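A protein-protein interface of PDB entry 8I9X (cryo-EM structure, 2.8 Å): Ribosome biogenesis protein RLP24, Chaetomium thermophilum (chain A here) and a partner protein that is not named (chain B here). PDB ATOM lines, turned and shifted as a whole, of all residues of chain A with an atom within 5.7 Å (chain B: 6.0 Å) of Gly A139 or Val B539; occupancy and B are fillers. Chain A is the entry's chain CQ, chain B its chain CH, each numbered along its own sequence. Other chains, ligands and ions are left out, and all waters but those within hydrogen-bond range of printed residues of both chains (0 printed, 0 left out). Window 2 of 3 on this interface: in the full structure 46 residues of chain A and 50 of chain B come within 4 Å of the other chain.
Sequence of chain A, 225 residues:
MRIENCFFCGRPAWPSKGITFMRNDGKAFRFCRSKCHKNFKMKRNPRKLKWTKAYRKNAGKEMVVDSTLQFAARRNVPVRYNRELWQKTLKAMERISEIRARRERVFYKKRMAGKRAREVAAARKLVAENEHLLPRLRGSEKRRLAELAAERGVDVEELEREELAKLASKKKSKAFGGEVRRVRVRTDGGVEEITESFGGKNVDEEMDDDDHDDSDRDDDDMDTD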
ATOM      1  N   LEU A 137     -18.612   8.158  13.278  1.00  0.00           N
ATOM      2  CA  LEU A 137     -18.882   7.516  14.559  1.00  0.00           C
ATOM      3  C   LEU A 137     -17.844   7.839  15.626  1.00  0.00           C
ATOM      4  O   LEU A 137     -17.374   8.977  15.731  1.00  0.00           O
ATOM      5  CB  LEU A 137     -18.958   5.997  14.389  1.00  0.00           C
ATOM      6  CG  LEU A 137     -20.284   5.413  13.904  1.00  0.00           C
ATOM      7  CD1 LEU A 137     -21.353   5.700  14.932  1.00  0.00           C
ATOM      8  CD2 LEU A 137     -20.683   5.891  12.516  1.00  0.00           C
ATOM      9  N   ARG A 138     -17.488   6.832  16.417  1.00  0.00           N
ATOM     10  CA  ARG A 138     -16.578   6.952  17.544  1.00  0.00           C
ATOM     11  C   ARG A 138     -16.082   5.550  17.867  1.00  0.00           C
ATOM     12  O   ARG A 138     -16.840   4.586  17.760  1.00  0.00           O
ATOM     13  CB  ARG A 138     -17.290   7.580  18.752  1.00  0.00           C
ATOM     14  CG  ARG A 138     -16.403   8.044  19.883  1.00  0.00           C
ATOM     15  CD  ARG A 138     -15.801   9.404  19.595  1.00  0.00           C
ATOM     16  NE  ARG A 138     -16.627  10.489  20.112  1.00  0.00           N
ATOM     17  CZ  ARG A 138     -16.502  11.014  21.323  1.00  0.00           C
ATOM     18  NH1 ARG A 138     -15.591  10.575  22.176  1.00  0.00           N
ATOM     19  NH2 ARG A 138     -17.314  12.002  21.687  1.00  0.00           N
ATOM     20  N   GLY A 139     -14.803   5.435  18.234  1.00  0.00           N
ATOM     21  CA  GLY A 139     -14.232   4.113  18.461  1.00  0.00           C
ATOM     22  C   GLY A 139     -14.838   3.404  19.658  1.00  0.00           C
ATOM     23  O   GLY A 139     -15.185   2.219  19.590  1.00  0.00           O
ATOM     24  N   SER A 140     -14.974   4.121  20.774  1.00  0.00           N
ATOM     25  CA  SER A 140     -15.624   3.539  21.943  1.00  0.00           C
ATOM     26  C   SER A 140     -17.090   3.253  21.656  1.00  0.00           C
ATOM     27  O   SER A 140     -17.656   2.280  22.168  1.00  0.00           O
ATOM     28  CB  SER A 140     -15.480   4.470  23.145  1.00  0.00           C
ATOM     29  OG  SER A 140     -16.183   5.683  22.939  1.00  0.00           O
ATOM     30  N   GLU A 141     -17.719   4.094  20.833  1.00  0.00           N
ATOM     31  CA  GLU A 141     -19.095   3.852  20.423  1.00  0.00           C
ATOM     32  C   GLU A 141     -19.197   2.541  19.653  1.00  0.00           C
ATOM     33  O   GLU A 141     -20.107   1.738  19.889  1.00  0.00           O
ATOM     34  CB  GLU A 141     -19.576   5.025  19.567  1.00  0.00           C
ATOM     35  CG  GLU A 141     -21.016   4.985  19.086  1.00  0.00           C
ATOM     36  CD  GLU A 141     -22.011   5.079  20.230  1.00  0.00           C
ATOM     37  OE1 GLU A 141     -21.652   5.643  21.284  1.00  0.00           O
ATOM     38  OE2 GLU A 141     -23.166   4.644  20.060  1.00  0.00           O
ATOM     39  N   LYS A 142     -18.254   2.306  18.737  1.00  0.00           N
ATOM     40  CA  LYS A 142     -18.216   1.054  17.989  1.00  0.00           C
ATOM     41  C   LYS A 142     -18.010  -0.138  18.909  1.00  0.00           C
ATOM     42  O   LYS A 142     -18.649  -1.179  18.734  1.00  0.00           O
ATOM     43  CB  LYS A 142     -17.104   1.102  16.940  1.00  0.00           C
ATOM     44  CG  LYS A 142     -17.293   2.144  15.857  1.00  0.00           C
ATOM     45  CD  LYS A 142     -18.341   1.708  14.853  1.00  0.00           C
ATOM     46  CE  LYS A 142     -17.800   0.594  13.969  1.00  0.00           C
ATOM     47  NZ  LYS A 142     -18.710   0.280  12.837  1.00  0.00           N
ATOM     48  N   ARG A 143     -17.109  -0.012  19.884  1.00  0.00           N
ATOM     49  CA  ARG A 143     -16.874  -1.127  20.800  1.00  0.00           C
ATOM     50  C   ARG A 143     -18.117  -1.438  21.630  1.00  0.00           C
ATOM     51  O   ARG A 143     -18.502  -2.609  21.780  1.00  0.00           O
ATOM     52  CB  ARG A 143     -15.682  -0.819  21.705  1.00  0.00           C
ATOM     53  CG  ARG A 143     -15.275  -1.970  22.609  1.00  0.00           C
ATOM     54  CD  ARG A 143     -14.045  -1.625  23.432  1.00  0.00           C
ATOM     55  NE  ARG A 143     -14.296  -0.535  24.367  1.00  0.00           N
ATOM     56  CZ  ARG A 143     -13.731   0.662  24.291  1.00  0.00           C
ATOM     57  NH1 ARG A 143     -12.873   0.962  23.329  1.00  0.00           N
ATOM     58  NH2 ARG A 143     -14.034   1.582  25.203  1.00  0.00           N
ATOM     59  N   ARG A 144     -18.764  -0.401  22.167  1.00  0.00           N
ATOM     60  CA  ARG A 144     -19.979  -0.593  22.946  1.00  0.00           C
ATOM     61  C   ARG A 144     -21.116  -1.176  22.121  1.00  0.00           C
ATOM     62  O   ARG A 144     -21.814  -2.068  22.612  1.00  0.00           O
ATOM     63  CB  ARG A 144     -20.414   0.732  23.577  1.00  0.00           C
ATOM     64  CG  ARG A 144     -21.408   0.577  24.720  1.00  0.00           C
ATOM     65  CD  ARG A 144     -22.831   0.881  24.283  1.00  0.00           C
ATOM     66  NE  ARG A 144     -22.989   2.272  23.877  1.00  0.00           N
ATOM     67  CZ  ARG A 144     -24.040   2.744  23.220  1.00  0.00           C
ATOM     68  NH1 ARG A 144     -25.050   1.962  22.879  1.00  0.00           N
ATOM     69  NH2 ARG A 144     -24.076   4.034  22.897  1.00  0.00           N
ATOM     70  N   LEU B 534      -8.424  11.036  18.703  1.00  0.00           N
ATOM     71  CA  LEU B 534      -8.290   9.763  17.962  1.00  0.00           C
ATOM     72  C   LEU B 534      -9.614   9.019  18.051  1.00  0.00           C
ATOM     73  O   LEU B 534      -9.947   8.321  17.086  1.00  0.00           O
ATOM     74  CB  LEU B 534      -7.133   8.958  18.556  1.00  0.00           C
ATOM     75  CG  LEU B 534      -5.837   8.974  17.748  1.00  0.00           C
ATOM     76  CD1 LEU B 534      -5.380  10.396  17.467  1.00  0.00           C
ATOM     77  CD2 LEU B 534      -4.747   8.193  18.462  1.00  0.00           C
ATOM     78  N   ASP B 535     -10.325   9.160  19.165  1.00  0.00           N
ATOM     79  CA  ASP B 535     -11.672   8.552  19.271  1.00  0.00           C
ATOM     80  C   ASP B 535     -12.598   9.241  18.277  1.00  0.00           C
ATOM     81  O   ASP B 535     -13.259   8.535  17.527  1.00  0.00           O
ATOM     82  CB  ASP B 535     -12.221   8.688  20.687  1.00  0.00           C
ATOM     83  CG  ASP B 535     -12.898   7.431  21.207  1.00  0.00           C
ATOM     84  OD1 ASP B 535     -12.757   6.375  20.560  1.00  0.00           O
ATOM     85  OD2 ASP B 535     -13.564   7.520  22.256  1.00  0.00           O
ATOM     86  N   GLN B 536     -12.657  10.572  18.305  1.00  0.00           N
ATOM     87  CA  GLN B 536     -13.510  11.343  17.368  1.00  0.00           C
ATOM     88  C   GLN B 536     -13.101  10.975  15.961  1.00  0.00           C
ATOM     89  O   GLN B 536     -13.961  10.997  15.076  1.00  0.00           O
ATOM     90  CB  GLN B 536     -13.329  12.840  17.577  1.00  0.00           C
ATOM     91  CG  GLN B 536     -13.968  13.349  18.859  1.00  0.00           C
ATOM     92  CD  GLN B 536     -13.532  14.751  19.202  1.00  0.00           C
ATOM     93  OE1 GLN B 536     -12.561  15.274  18.657  1.00  0.00           O
ATOM     94  NE2 GLN B 536     -14.249  15.373  20.122  1.00  0.00           N
ATOM     95  N   LEU B 537     -11.819  10.683  15.772  1.00  0.00           N
ATOM     96  CA  LEU B 537     -11.410  10.196  14.462  1.00  0.00           C
ATOM     97  C   LEU B 537     -11.809   8.746  14.220  1.00  0.00           C
ATOM     98  O   LEU B 537     -11.825   8.307  13.066  1.00  0.00           O
ATOM     99  CB  LEU B 537      -9.895  10.342  14.286  1.00  0.00           C
ATOM    100  CG  LEU B 537      -9.348  11.769  14.245  1.00  0.00           C
ATOM    101  CD1 LEU B 537      -7.828  11.758  14.209  1.00  0.00           C
ATOM    102  CD2 LEU B 537      -9.910  12.513  13.046  1.00  0.00           C
ATOM    103  N   GLY B 538     -12.269   8.034  15.235  1.00  0.00           N
ATOM    104  CA  GLY B 538     -12.776   6.673  14.982  1.00  0.00           C
ATOM    105  C   GLY B 538     -11.676   5.652  15.052  1.00  0.00           C
ATOM    106  O   GLY B 538     -11.401   5.024  14.021  1.00  0.00           O
ATOM    107  N   VAL B 539     -11.085   5.484  16.228  1.00  0.00           N
ATOM    108  CA  VAL B 539      -9.954   4.538  16.419  1.00  0.00           C
ATOM    109  C   VAL B 539     -10.143   3.894  17.790  1.00  0.00           C
ATOM    110  O   VAL B 539     -10.571   4.613  18.715  1.00  0.00           O
ATOM    111  CB  VAL B 539      -8.616   5.293  16.343  1.00  0.00           C
ATOM    112  CG1 VAL B 539      -7.462   4.510  16.949  1.00  0.00           C
ATOM    113  CG2 VAL B 539      -8.275   5.735  14.929  1.00  0.00           C
ATOM    114  N   ASP B 540      -9.835   2.601  17.929  1.00  0.00           N
ATOM    115  CA  ASP B 540      -9.917   1.966  19.263  1.00  0.00           C
ATOM    116  C   ASP B 540      -8.739   2.463  20.098  1.00  0.00           C
ATOM    117  O   ASP B 540      -7.613   2.003  19.867  1.00  0.00           O
ATOM    118  CB  ASP B 540      -9.937   0.445  19.141  1.00  0.00           C
ATOM    119  CG  ASP B 540     -10.383  -0.259  20.411  1.00  0.00           C
ATOM    120  OD1 ASP B 540     -10.905   0.426  21.312  1.00  0.00           O
ATOM    121  OD2 ASP B 540     -10.203  -1.490  20.489  1.00  0.00           O
ATOM    122  N   THR B 541      -8.994   3.382  21.020  1.00  0.00           N
ATOM    123  CA  THR B 541      -7.914   3.844  21.914  1.00  0.00           C
ATOM    124  C   THR B 541      -7.597   2.715  22.892  1.00  0.00           C
ATOM    125  O   THR B 541      -6.441   2.623  23.327  1.00  0.00           O
ATOM    126  CB  THR B 541      -8.317   5.144  22.614  1.00  0.00           C
ATOM    127  OG1 THR B 541      -9.448   4.886  23.447  1.00  0.00           O
ATOM    128  CG2 THR B 541      -8.648   6.247  21.634  1.00  0.00           C
ATOM    129  N   GLU B 542      -8.595   1.883  23.207  1.00  0.00           N
ATOM    130  CA  GLU B 542      -8.402   0.767  24.167  1.00  0.00           C
ATOM    131  C   GLU B 542      -7.570  -0.334  23.506  1.00  0.00           C
ATOM    132  O   GLU B 542      -7.075  -1.208  24.243  1.00  0.00           O
ATOM    133  CB  GLU B 542      -9.753   0.256  24.661  1.00  0.00           C
ATOM    134  CG  GLU B 542     -10.259   0.987  25.894  1.00  0.00           C
ATOM    135  CD  GLU B 542     -10.558   2.466  25.714  1.00  0.00           C
ATOM    136  OE1 GLU B 542     -11.074   2.842  24.642  1.00  0.00           O
ATOM    137  OE2 GLU B 542     -10.267   3.242  26.646  1.00  0.00           O
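Printed residues of chain A that touch a printed residue of chain B: Arg A138, Gly A139, Ser A140 and Arg A143. Printed residues of chain B that touch a printed residue of chain A: Asp B535, Gln B536, Val B539, Asp B540 and Glu B542. Among the printed residues, Asp or Glu carboxylates within 4 Å of a Lys or Arg side-chain nitrogen of the other chain: Arg A138 with Asp B535 (3.7 Å), Arg A143 with Asp B540 (2.9 Å) and Arg A143 with Glu B542 (2.9 Å).
Among the printed residues, merely in contact across the chains: Arg A138 with Gln B536 (3.6 Å) and Gly A139 with Val B539 (3.7 Å).
O of Leu B534 is in hydrogen-bond range of N of Val B539 (3.2 Å). N of Glu B542 sits close to OD1 of Asp B540 (3.3 Å). The side-chain hydroxyl (OG1) of Thr B541 is in hydrogen-bond range of the side-chain carboxylate (OE1) of Glu B542, 2.9 Å away.
Leu A137 touches none of the printed residues of chain B. Of the printed residues of chain B, Arg A138 touches Asp B535 (3.4 Å) and Gln B536 (3.6 Å). Gly A139 touches just these residues of chain B: Asp B535 (3.2 Å) and Val B539 (3.7 Å). Printed residues of chain B within 4 Å of Ser A140: Asp B535 (3.2 Å). Lys A142 touches none of the printed residues of chain B. Of the printed residues of chain B, Arg A143 touches Asp B540 and Glu B542. Of the printed residues of chain A, Asp B535 touches Arg A138 (3.4 Å), Gly A139 (3.2 Å) and Ser A140 (3.2 Å). Of the printed residues of chain A, Gln B536 touches Arg A138. The nearest residue of chain B that does not touch Gly A139 is Gly B538 (4.03 Å). The nearest residue of chain A that does not touch Val B539 is Ser A140 (4.9 Å).
OD2 of Asp B535 lies within salt-bridge range of NH1 of Arg A138 (3.7 Å). N of Gly A139 is in hydrogen-bond range of OD1 of Asp B535, at 3.2 Å. The side-chain carboxylate (OD1) of Asp B535 is in hydrogen-bond range of the backbone NH (N) of Ser A140 (3.2 Å). OD1 of Asp B540 lies within salt-bridge range of NH1 of Arg A143, at 2.9 Å. The guanidinium group (NH1) of Arg A143 lies within salt-bridge range of the side-chain carboxylate (OE1) of Glu B542 (2.9 Å).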
